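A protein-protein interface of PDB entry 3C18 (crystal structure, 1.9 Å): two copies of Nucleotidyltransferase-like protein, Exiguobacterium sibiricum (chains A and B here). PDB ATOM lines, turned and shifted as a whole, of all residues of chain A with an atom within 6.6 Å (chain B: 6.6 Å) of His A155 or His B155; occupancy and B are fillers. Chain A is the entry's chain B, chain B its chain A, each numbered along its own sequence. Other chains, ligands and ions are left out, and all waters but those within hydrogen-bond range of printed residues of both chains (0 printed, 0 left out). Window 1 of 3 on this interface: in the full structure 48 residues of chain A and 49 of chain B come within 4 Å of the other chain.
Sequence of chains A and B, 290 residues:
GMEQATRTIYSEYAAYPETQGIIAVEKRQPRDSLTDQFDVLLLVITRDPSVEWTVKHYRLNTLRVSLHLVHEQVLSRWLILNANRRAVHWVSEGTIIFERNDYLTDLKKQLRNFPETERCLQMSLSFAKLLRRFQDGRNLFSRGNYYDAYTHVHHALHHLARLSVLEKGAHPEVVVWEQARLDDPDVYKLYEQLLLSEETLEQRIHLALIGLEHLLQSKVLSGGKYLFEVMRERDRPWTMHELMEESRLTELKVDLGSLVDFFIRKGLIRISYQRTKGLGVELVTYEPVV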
ATOM      1  N   LYS A 129     -11.522 -12.953  -9.876  1.00  0.00           N
ATOM      2  CA  LYS A 129     -11.245 -13.283  -8.470  1.00  0.00           C
ATOM      3  C   LYS A 129     -12.294 -14.265  -7.946  1.00  0.00           C
ATOM      4  O   LYS A 129     -12.006 -15.207  -7.209  1.00  0.00           O
ATOM      5  CB  LYS A 129     -11.166 -12.015  -7.602  1.00  0.00           C
ATOM      6  CG  LYS A 129      -9.825 -11.277  -7.670  1.00  0.00           C
ATOM      7  N   LEU A 130     -13.522 -14.042  -8.372  1.00  0.00           N
ATOM      8  CA  LEU A 130     -14.646 -14.931  -8.007  1.00  0.00           C
ATOM      9  C   LEU A 130     -14.388 -16.349  -8.509  1.00  0.00           C
ATOM     10  O   LEU A 130     -14.546 -17.343  -7.799  1.00  0.00           O
ATOM     11  CB  LEU A 130     -15.948 -14.415  -8.634  1.00  0.00           C
ATOM     12  CG  LEU A 130     -17.112 -15.380  -8.822  1.00  0.00           C
ATOM     13  CD1 LEU A 130     -17.639 -15.891  -7.511  1.00  0.00           C
ATOM     14  CD2 LEU A 130     -18.184 -14.639  -9.565  1.00  0.00           C
ATOM     15  N   ARG A 133     -11.461 -18.029  -6.505  1.00  0.00           N
ATOM     16  CA  ARG A 133     -11.878 -18.388  -5.139  1.00  0.00           C
ATOM     17  C   ARG A 133     -12.861 -19.566  -5.189  1.00  0.00           C
ATOM     18  O   ARG A 133     -12.822 -20.481  -4.370  1.00  0.00           O
ATOM     19  CB  ARG A 133     -12.518 -17.197  -4.389  1.00  0.00           C
ATOM     20  CG  ARG A 133     -11.572 -16.091  -4.080  1.00  0.00           C
ATOM     21  CD  ARG A 133     -10.572 -16.418  -2.982  1.00  0.00           C
ATOM     22  NE  ARG A 133      -9.586 -17.414  -3.395  1.00  0.00           N
ATOM     23  CZ  ARG A 133      -8.511 -17.154  -4.130  1.00  0.00           C
ATOM     24  NH1 ARG A 133      -8.273 -15.925  -4.560  1.00  0.00           N
ATOM     25  NH2 ARG A 133      -7.671 -18.130  -4.447  1.00  0.00           N
ATOM     26  N   TYR A 150     -14.102 -23.062   3.464  1.00  0.00           N
ATOM     27  CA  TYR A 150     -15.044 -22.038   3.914  1.00  0.00           C
ATOM     28  C   TYR A 150     -14.464 -20.662   3.667  1.00  0.00           C
ATOM     29  O   TYR A 150     -15.167 -19.726   3.354  1.00  0.00           O
ATOM     30  CB  TYR A 150     -15.412 -22.223   5.387  1.00  0.00           C
ATOM     31  CG  TYR A 150     -16.436 -21.247   5.924  1.00  0.00           C
ATOM     32  CD1 TYR A 150     -16.075 -19.965   6.301  1.00  0.00           C
ATOM     33  CD2 TYR A 150     -17.741 -21.635   6.134  1.00  0.00           C
ATOM     34  CE1 TYR A 150     -17.015 -19.083   6.842  1.00  0.00           C
ATOM     35  CE2 TYR A 150     -18.679 -20.763   6.657  1.00  0.00           C
ATOM     36  CZ  TYR A 150     -18.315 -19.489   6.998  1.00  0.00           C
ATOM     37  OH  TYR A 150     -19.245 -18.627   7.529  1.00  0.00           O
ATOM     38  N   THR A 151     -13.149 -20.583   3.711  1.00  0.00           N
ATOM     39  CA  THR A 151     -12.447 -19.327   3.549  1.00  0.00           C
ATOM     40  C   THR A 151     -12.590 -18.828   2.135  1.00  0.00           C
ATOM     41  O   THR A 151     -12.831 -17.658   1.891  1.00  0.00           O
ATOM     42  CB  THR A 151     -10.937 -19.485   3.875  1.00  0.00           C
ATOM     43  OG1 THR A 151     -10.774 -19.735   5.278  1.00  0.00           O
ATOM     44  CG2 THR A 151     -10.181 -18.219   3.509  1.00  0.00           C
ATOM     45  N   HIS A 152     -12.447 -19.740   1.188  1.00  0.00           N
ATOM     46  CA  HIS A 152     -12.455 -19.360  -0.224  1.00  0.00           C
ATOM     47  C   HIS A 152     -13.842 -19.164  -0.712  1.00  0.00           C
ATOM     48  O   HIS A 152     -14.087 -18.325  -1.554  1.00  0.00           O
ATOM     49  CB  HIS A 152     -11.731 -20.387  -1.091  1.00  0.00           C
ATOM     50  CG  HIS A 152     -10.271 -20.398  -0.851  1.00  0.00           C
ATOM     51  ND1 HIS A 152      -9.414 -19.535  -1.494  1.00  0.00           N
ATOM     52  CD2 HIS A 152      -9.518 -21.106   0.020  1.00  0.00           C
ATOM     53  CE1 HIS A 152      -8.186 -19.731  -1.047  1.00  0.00           C
ATOM     54  NE2 HIS A 152      -8.222 -20.682  -0.131  1.00  0.00           N
ATOM     55  N   VAL A 153     -14.744 -19.979  -0.197  1.00  0.00           N
ATOM     56  CA  VAL A 153     -16.146 -19.871  -0.582  1.00  0.00           C
ATOM     57  C   VAL A 153     -16.665 -18.521  -0.110  1.00  0.00           C
ATOM     58  O   VAL A 153     -17.395 -17.817  -0.795  1.00  0.00           O
ATOM     59  CB  VAL A 153     -17.005 -21.012  -0.003  1.00  0.00           C
ATOM     60  CG1 VAL A 153     -18.480 -20.725  -0.229  1.00  0.00           C
ATOM     61  CG2 VAL A 153     -16.609 -22.307  -0.663  1.00  0.00           C
ATOM     62  N   HIS A 154     -16.174 -18.133   1.043  1.00  0.00           N
ATOM     63  CA  HIS A 154     -16.600 -16.895   1.656  1.00  0.00           C
ATOM     64  C   HIS A 154     -16.123 -15.704   0.848  1.00  0.00           C
ATOM     65  O   HIS A 154     -16.881 -14.794   0.551  1.00  0.00           O
ATOM     66  CB  HIS A 154     -16.088 -16.819   3.080  1.00  0.00           C
ATOM     67  CG  HIS A 154     -16.506 -15.583   3.790  1.00  0.00           C
ATOM     68  ND1 HIS A 154     -15.787 -14.415   3.699  1.00  0.00           N
ATOM     69  CD2 HIS A 154     -17.569 -15.320   4.585  1.00  0.00           C
ATOM     70  CE1 HIS A 154     -16.386 -13.479   4.414  1.00  0.00           C
ATOM     71  NE2 HIS A 154     -17.462 -14.002   4.972  1.00  0.00           N
ATOM     72  N   HIS A 155     -14.862 -15.738   0.470  1.00  0.00           N
ATOM     73  CA  HIS A 155     -14.249 -14.671  -0.349  1.00  0.00           C
ATOM     74  C   HIS A 155     -14.897 -14.620  -1.710  1.00  0.00           C
ATOM     75  O   HIS A 155     -15.055 -13.560  -2.314  1.00  0.00           O
ATOM     76  CB  HIS A 155     -12.749 -14.899  -0.533  1.00  0.00           C
ATOM     77  CG  HIS A 155     -11.926 -14.565   0.668  1.00  0.00           C
ATOM     78  ND1 HIS A 155     -12.309 -14.890   1.953  1.00  0.00           N
ATOM     79  CD2 HIS A 155     -10.722 -13.964   0.777  1.00  0.00           C
ATOM     80  CE1 HIS A 155     -11.378 -14.494   2.800  1.00  0.00           C
ATOM     81  NE2 HIS A 155     -10.402 -13.938   2.110  1.00  0.00           N
ATOM     82  N   ALA A 156     -15.319 -15.787  -2.187  1.00  0.00           N
ATOM     83  CA  ALA A 156     -15.965 -15.882  -3.508  1.00  0.00           C
ATOM     84  C   ALA A 156     -17.276 -15.126  -3.492  1.00  0.00           C
ATOM     85  O   ALA A 156     -17.599 -14.418  -4.423  1.00  0.00           O
ATOM     86  CB  ALA A 156     -16.205 -17.335  -3.956  1.00  0.00           C
ATOM     87  N   LEU A 157     -18.038 -15.294  -2.411  1.00  0.00           N
ATOM     88  CA  LEU A 157     -19.342 -14.627  -2.294  1.00  0.00           C
ATOM     89  C   LEU A 157     -19.142 -13.118  -2.256  1.00  0.00           C
ATOM     90  O   LEU A 157     -19.914 -12.354  -2.799  1.00  0.00           O
ATOM     91  CB  LEU A 157     -20.084 -15.078  -1.048  1.00  0.00           C
ATOM     92  CG  LEU A 157     -20.629 -16.485  -1.175  1.00  0.00           C
ATOM     93  CD1 LEU A 157     -21.163 -17.025   0.180  1.00  0.00           C
ATOM     94  CD2 LEU A 157     -21.729 -16.508  -2.239  1.00  0.00           C
ATOM     95  N   HIS A 158     -18.052 -12.705  -1.648  1.00  0.00           N
ATOM     96  CA  HIS A 158     -17.770 -11.286  -1.516  1.00  0.00           C
ATOM     97  C   HIS A 158     -17.515 -10.659  -2.881  1.00  0.00           C
ATOM     98  O   HIS A 158     -18.016  -9.565  -3.180  1.00  0.00           O
ATOM     99  CB  HIS A 158     -16.601 -11.050  -0.572  1.00  0.00           C
ATOM    100  CG  HIS A 158     -16.472  -9.631  -0.141  1.00  0.00           C
ATOM    101  ND1 HIS A 158     -15.318  -8.902  -0.307  1.00  0.00           N
ATOM    102  CD2 HIS A 158     -17.375  -8.787   0.413  1.00  0.00           C
ATOM    103  CE1 HIS A 158     -15.504  -7.676   0.151  1.00  0.00           C
ATOM    104  NE2 HIS A 158     -16.750  -7.576   0.575  1.00  0.00           N
ATOM    105  N   HIS A 159     -16.747 -11.359  -3.720  1.00  0.00           N
ATOM    106  CA  HIS A 159     -16.424 -10.851  -5.071  1.00  0.00           C
ATOM    107  C   HIS A 159     -17.685 -10.833  -5.919  1.00  0.00           C
ATOM    108  O   HIS A 159     -17.884  -9.977  -6.782  1.00  0.00           O
ATOM    109  CB  HIS A 159     -15.358 -11.706  -5.762  1.00  0.00           C
ATOM    110  CG  HIS A 159     -14.014 -11.658  -5.114  1.00  0.00           C
ATOM    111  ND1 HIS A 159     -13.330 -10.480  -4.926  1.00  0.00           N
ATOM    112  CD2 HIS A 159     -13.194 -12.643  -4.677  1.00  0.00           C
ATOM    113  CE1 HIS A 159     -12.169 -10.735  -4.345  1.00  0.00           C
ATOM    114  NE2 HIS A 159     -12.046 -12.040  -4.205  1.00  0.00           N
ATOM    115  N   LEU A 160     -18.560 -11.791  -5.648  1.00  0.00           N
ATOM    116  CA  LEU A 160     -19.809 -11.920  -6.392  1.00  0.00           C
ATOM    117  C   LEU A 160     -20.729 -10.779  -6.050  1.00  0.00           C
ATOM    118  O   LEU A 160     -21.459 -10.258  -6.893  1.00  0.00           O
ATOM    119  CB  LEU A 160     -20.487 -13.235  -6.047  1.00  0.00           C
ATOM    120  CG  LEU A 160     -21.816 -13.580  -6.702  1.00  0.00           C
ATOM    121  CD1 LEU A 160     -21.810 -13.567  -8.228  1.00  0.00           C
ATOM    122  CD2 LEU A 160     -22.220 -14.955  -6.177  1.00  0.00           C
ATOM    123  N   LYS B 129      -1.986  -6.577   7.629  1.00  0.00           N
ATOM    124  CA  LYS B 129      -3.301  -6.861   7.026  1.00  0.00           C
ATOM    125  C   LYS B 129      -4.292  -7.287   8.097  1.00  0.00           C
ATOM    126  O   LYS B 129      -5.505  -6.977   8.043  1.00  0.00           O
ATOM    127  CB  LYS B 129      -3.180  -7.950   5.967  1.00  0.00           C
ATOM    128  CG  LYS B 129      -2.383  -7.590   4.729  1.00  0.00           C
ATOM    129  CD  LYS B 129      -2.902  -6.347   4.060  1.00  0.00           C
ATOM    130  N   LEU B 130      -3.784  -8.023   9.068  1.00  0.00           N
ATOM    131  CA  LEU B 130      -4.638  -8.438  10.218  1.00  0.00           C
ATOM    132  C   LEU B 130      -5.190  -7.193  10.909  1.00  0.00           C
ATOM    133  O   LEU B 130      -6.373  -7.092  11.263  1.00  0.00           O
ATOM    134  CB  LEU B 130      -3.824  -9.256  11.224  1.00  0.00           C
ATOM    135  CG  LEU B 130      -4.288  -9.439  12.662  1.00  0.00           C
ATOM    136  CD1 LEU B 130      -5.641 -10.113  12.766  1.00  0.00           C
ATOM    137  CD2 LEU B 130      -3.188 -10.245  13.407  1.00  0.00           C
ATOM    138  N   ARG B 133      -7.798  -5.301   8.731  1.00  0.00           N
ATOM    139  CA  ARG B 133      -9.087  -6.030   8.684  1.00  0.00           C
ATOM    140  C   ARG B 133      -9.819  -5.944  10.025  1.00  0.00           C
ATOM    141  O   ARG B 133     -11.049  -5.771  10.094  1.00  0.00           O
ATOM    142  CB  ARG B 133      -8.903  -7.486   8.227  1.00  0.00           C
ATOM    143  CG  ARG B 133      -8.409  -7.636   6.802  1.00  0.00           C
ATOM    144  CD  ARG B 133      -9.458  -7.360   5.720  1.00  0.00           C
ATOM    145  NE  ARG B 133      -9.791  -5.947   5.572  1.00  0.00           N
ATOM    146  CZ  ARG B 133      -9.015  -5.043   4.973  1.00  0.00           C
ATOM    147  NH1 ARG B 133      -7.856  -5.392   4.458  1.00  0.00           N
ATOM    148  NH2 ARG B 133      -9.382  -3.777   4.931  1.00  0.00           N
ATOM    149  N   TYR B 150     -18.581  -8.967   9.479  1.00  0.00           N
ATOM    150  CA  TYR B 150     -18.261 -10.400   9.445  1.00  0.00           C
ATOM    151  C   TYR B 150     -17.238 -10.674   8.402  1.00  0.00           C
ATOM    152  O   TYR B 150     -16.289 -11.415   8.624  1.00  0.00           O
ATOM    153  CB  TYR B 150     -19.480 -11.241   9.132  1.00  0.00           C
ATOM    154  CG  TYR B 150     -19.266 -12.729   9.264  1.00  0.00           C
ATOM    155  CD1 TYR B 150     -18.611 -13.452   8.277  1.00  0.00           C
ATOM    156  CD2 TYR B 150     -19.683 -13.404  10.401  1.00  0.00           C
ATOM    157  CE1 TYR B 150     -18.403 -14.838   8.396  1.00  0.00           C
ATOM    158  CE2 TYR B 150     -19.491 -14.797  10.532  1.00  0.00           C
ATOM    159  CZ  TYR B 150     -18.867 -15.511   9.531  1.00  0.00           C
ATOM    160  OH  TYR B 150     -18.682 -16.883   9.663  1.00  0.00           O
ATOM    161  N   THR B 151     -17.393 -10.019   7.260  1.00  0.00           N
ATOM    162  CA  THR B 151     -16.457 -10.210   6.161  1.00  0.00           C
ATOM    163  C   THR B 151     -15.039  -9.864   6.583  1.00  0.00           C
ATOM    164  O   THR B 151     -14.111 -10.615   6.349  1.00  0.00           O
ATOM    165  CB  THR B 151     -16.864  -9.422   4.878  1.00  0.00           C
ATOM    166  OG1 THR B 151     -18.144  -9.881   4.425  1.00  0.00           O
ATOM    167  CG2 THR B 151     -15.869  -9.667   3.799  1.00  0.00           C
ATOM    168  N   HIS B 152     -14.875  -8.720   7.237  1.00  0.00           N
ATOM    169  CA  HIS B 152     -13.546  -8.255   7.655  1.00  0.00           C
ATOM    170  C   HIS B 152     -12.999  -9.044   8.822  1.00  0.00           C
ATOM    171  O   HIS B 152     -11.827  -9.370   8.861  1.00  0.00           O
ATOM    172  CB  HIS B 152     -13.551  -6.754   7.915  1.00  0.00           C
ATOM    173  CG  HIS B 152     -13.775  -5.969   6.669  1.00  0.00           C
ATOM    174  ND1 HIS B 152     -12.748  -5.345   5.989  1.00  0.00           N
ATOM    175  CD2 HIS B 152     -14.887  -5.779   5.921  1.00  0.00           C
ATOM    176  CE1 HIS B 152     -13.230  -4.761   4.908  1.00  0.00           C
ATOM    177  NE2 HIS B 152     -14.519  -5.019   4.834  1.00  0.00           N
ATOM    178  N   VAL B 153     -13.883  -9.419   9.729  1.00  0.00           N
ATOM    179  CA  VAL B 153     -13.449 -10.189  10.882  1.00  0.00           C
ATOM    180  C   VAL B 153     -12.898 -11.526  10.413  1.00  0.00           C
ATOM    181  O   VAL B 153     -11.866 -12.007  10.893  1.00  0.00           O
ATOM    182  CB  VAL B 153     -14.556 -10.409  11.904  1.00  0.00           C
ATOM    183  CG1 VAL B 153     -14.212 -11.588  12.771  1.00  0.00           C
ATOM    184  CG2 VAL B 153     -14.713  -9.131  12.734  1.00  0.00           C
ATOM    185  N   HIS B 154     -13.580 -12.101   9.433  1.00  0.00           N
ATOM    186  CA  HIS B 154     -13.206 -13.422   8.896  1.00  0.00           C
ATOM    187  C   HIS B 154     -11.843 -13.316   8.221  1.00  0.00           C
ATOM    188  O   HIS B 154     -10.945 -14.121   8.429  1.00  0.00           O
ATOM    189  CB  HIS B 154     -14.285 -13.923   7.926  1.00  0.00           C
ATOM    190  CG  HIS B 154     -13.928 -15.192   7.238  1.00  0.00           C
ATOM    191  ND1 HIS B 154     -13.122 -15.224   6.124  1.00  0.00           N
ATOM    192  CD2 HIS B 154     -14.241 -16.481   7.516  1.00  0.00           C
ATOM    193  CE1 HIS B 154     -12.937 -16.477   5.756  1.00  0.00           C
ATOM    194  NE2 HIS B 154     -13.616 -17.258   6.572  1.00  0.00           N
ATOM    195  N   HIS B 155     -11.665 -12.268   7.449  1.00  0.00           N
ATOM    196  CA  HIS B 155     -10.398 -12.048   6.758  1.00  0.00           C
ATOM    197  C   HIS B 155      -9.286 -11.842   7.772  1.00  0.00           C
ATOM    198  O   HIS B 155      -8.186 -12.366   7.638  1.00  0.00           O
ATOM    199  CB  HIS B 155     -10.484 -10.843   5.827  1.00  0.00           C
ATOM    200  CG  HIS B 155     -11.383 -11.042   4.644  1.00  0.00           C
ATOM    201  ND1 HIS B 155     -11.355 -10.209   3.550  1.00  0.00           N
ATOM    202  CD2 HIS B 155     -12.330 -11.976   4.379  1.00  0.00           C
ATOM    203  CE1 HIS B 155     -12.253 -10.608   2.667  1.00  0.00           C
ATOM    204  NE2 HIS B 155     -12.851 -11.686   3.141  1.00  0.00           N
ATOM    205  N   ALA B 156      -9.578 -11.078   8.813  1.00  0.00           N
ATOM    206  CA  ALA B 156      -8.559 -10.813   9.851  1.00  0.00           C
ATOM    207  C   ALA B 156      -8.135 -12.111  10.456  1.00  0.00           C
ATOM    208  O   ALA B 156      -6.977 -12.344  10.751  1.00  0.00           O
ATOM    209  CB  ALA B 156      -9.112  -9.889  10.970  1.00  0.00           C
ATOM    210  N   LEU B 157      -9.093 -12.978  10.682  1.00  0.00           N
ATOM    211  CA  LEU B 157      -8.774 -14.288  11.301  1.00  0.00           C
ATOM    212  C   LEU B 157      -7.868 -15.116  10.393  1.00  0.00           C
ATOM    213  O   LEU B 157      -6.982 -15.830  10.834  1.00  0.00           O
ATOM    214  CB  LEU B 157     -10.044 -15.070  11.603  1.00  0.00           C
ATOM    215  CG  LEU B 157     -10.798 -14.639  12.855  1.00  0.00           C
ATOM    216  CD1 LEU B 157     -12.183 -15.240  12.877  1.00  0.00           C
ATOM    217  CD2 LEU B 157     -10.051 -15.024  14.070  1.00  0.00           C
ATOM    218  N   HIS B 158      -8.086 -14.971   9.106  1.00  0.00           N
ATOM    219  CA  HIS B 158      -7.292 -15.690   8.105  1.00  0.00           C
ATOM    220  C   HIS B 158      -5.852 -15.143   8.140  1.00  0.00           C
ATOM    221  O   HIS B 158      -4.893 -15.881   8.125  1.00  0.00           O
ATOM    222  CB  HIS B 158      -7.880 -15.534   6.705  1.00  0.00           C
ATOM    223  CG  HIS B 158      -7.257 -16.440   5.703  1.00  0.00           C
ATOM    224  ND1 HIS B 158      -6.664 -15.987   4.549  1.00  0.00           N
ATOM    225  CD2 HIS B 158      -7.100 -17.785   5.709  1.00  0.00           C
ATOM    226  CE1 HIS B 158      -6.182 -17.019   3.878  1.00  0.00           C
ATOM    227  NE2 HIS B 158      -6.440 -18.121   4.558  1.00  0.00           N
ATOM    228  N   HIS B 159      -5.702 -13.833   8.230  1.00  0.00           N
ATOM    229  CA  HIS B 159      -4.339 -13.267   8.339  1.00  0.00           C
ATOM    230  C   HIS B 159      -3.634 -13.690   9.607  1.00  0.00           C
ATOM    231  O   HIS B 159      -2.400 -13.845   9.631  1.00  0.00           O
ATOM    232  CB  HIS B 159      -4.335 -11.745   8.232  1.00  0.00           C
ATOM    233  CG  HIS B 159      -4.712 -11.271   6.873  1.00  0.00           C
ATOM    234  ND1 HIS B 159      -4.015 -11.639   5.745  1.00  0.00           N
ATOM    235  CD2 HIS B 159      -5.744 -10.509   6.453  1.00  0.00           C
ATOM    236  CE1 HIS B 159      -4.586 -11.085   4.693  1.00  0.00           C
ATOM    237  NE2 HIS B 159      -5.636 -10.402   5.097  1.00  0.00           N
ATOM    238  N   LEU B 160      -4.416 -13.866  10.662  1.00  0.00           N
ATOM    239  CA  LEU B 160      -3.889 -14.253  11.986  1.00  0.00           C
ATOM    240  C   LEU B 160      -3.361 -15.689  11.972  1.00  0.00           C
ATOM    241  O   LEU B 160      -2.366 -16.030  12.622  1.00  0.00           O
ATOM    242  CB  LEU B 160      -4.978 -14.097  13.051  1.00  0.00           C
ATOM    243  CG  LEU B 160      -4.701 -14.459  14.524  1.00  0.00           C
ATOM    244  CD1 LEU B 160      -3.729 -13.548  15.181  1.00  0.00           C
ATOM    245  CD2 LEU B 160      -5.995 -14.494  15.338  1.00  0.00           C
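Tyr A150 touches its own counterpart, Tyr B150. Thr A151 touches His B154, and with the chains exchanged His A154 touches Thr B151. His B154 touches its own counterpart, His A154. His B155 touches its own counterpart, His A155. Positions printed for both chains: 129, 130, 133, 150, 151, 152, 153, 154, 155, 156, 157, 158, 159 and 160.
OH of Tyr B150 sits at hydrogen-bond distance from OH of Tyr A150 (2.8 Å). A ring nitrogen (NE2) of His B155 lies close to a ring nitrogen (ND1) of His A155 (3.5 Å).
Printed residues of chain B within 4 Å of Tyr A150: Tyr B150 (2.8 Å) and His B154 (3.7 Å). Of the printed residues of chain B, Thr A151 touches His B154 (3.6 Å) and His B158 (3.8 Å). Of the printed residues of chain B, His A154 touches Tyr B150, Thr B151 and His B154. Printed residues of chain B within 4 Å of His A155: His B154 (3.8 Å) and His B155 (3.1 Å). Lys B129 touches none of the printed residues of chain A. Printed residues of chain A within 4 Å of His B155: His A155. Leu B157 touches none of the printed residues of chain A. The nearest printed residue of chain B that does not touch His A155 is His B158 (4.9 Å). The nearest printed residue of chain A that does not touch His B158 is His A155 (4.9 Å).
Of the 14 printed residues of chain A, 5 touch a printed residue of chain B. Printed residues of chain A that touch a printed residue of chain B: Tyr A150, Thr A151, His A154, His A155 and His A158. Hydrophobic or aromatic side chains of chain A that line the printed part of chain B: Tyr A150, His A154, His A155 and His A158. Along chain A the printed residues that touch a printed residue of chain B span positions 150 to 158. Hydrophobic or aromatic side chains of chain B that line the printed part of chain A: Tyr B150, His B154, His B155 and His B158. Among the printed residues, 10 pairs touch across the chains. Among the printed residues, no Asp or Glu carboxylate lies within 4 Å of a Lys or Arg side-chain nitrogen of the other chain.
CD1 of Tyr A150 touches NE2 of His B154 (3.7 Å). CE1 of His B154 touches CA of Thr A151, 3.6 Å away. Thr A151 touches His B158 (CG2 to CD2, 3.8 Å). NE2 of His A154 touches CD1 of Tyr B150, at 3.5 Å. CE1 of His A154 touches CA of Thr B151, at 3.7 Å. ND1 of His A154 touches ND1 of His B154, at 3.7 Å. His A155 touches His B154. His A158 touches Thr B151.
O of Thr A151 sits at hydrogen-bond distance from ND1 of His A155 (2.8 Å).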
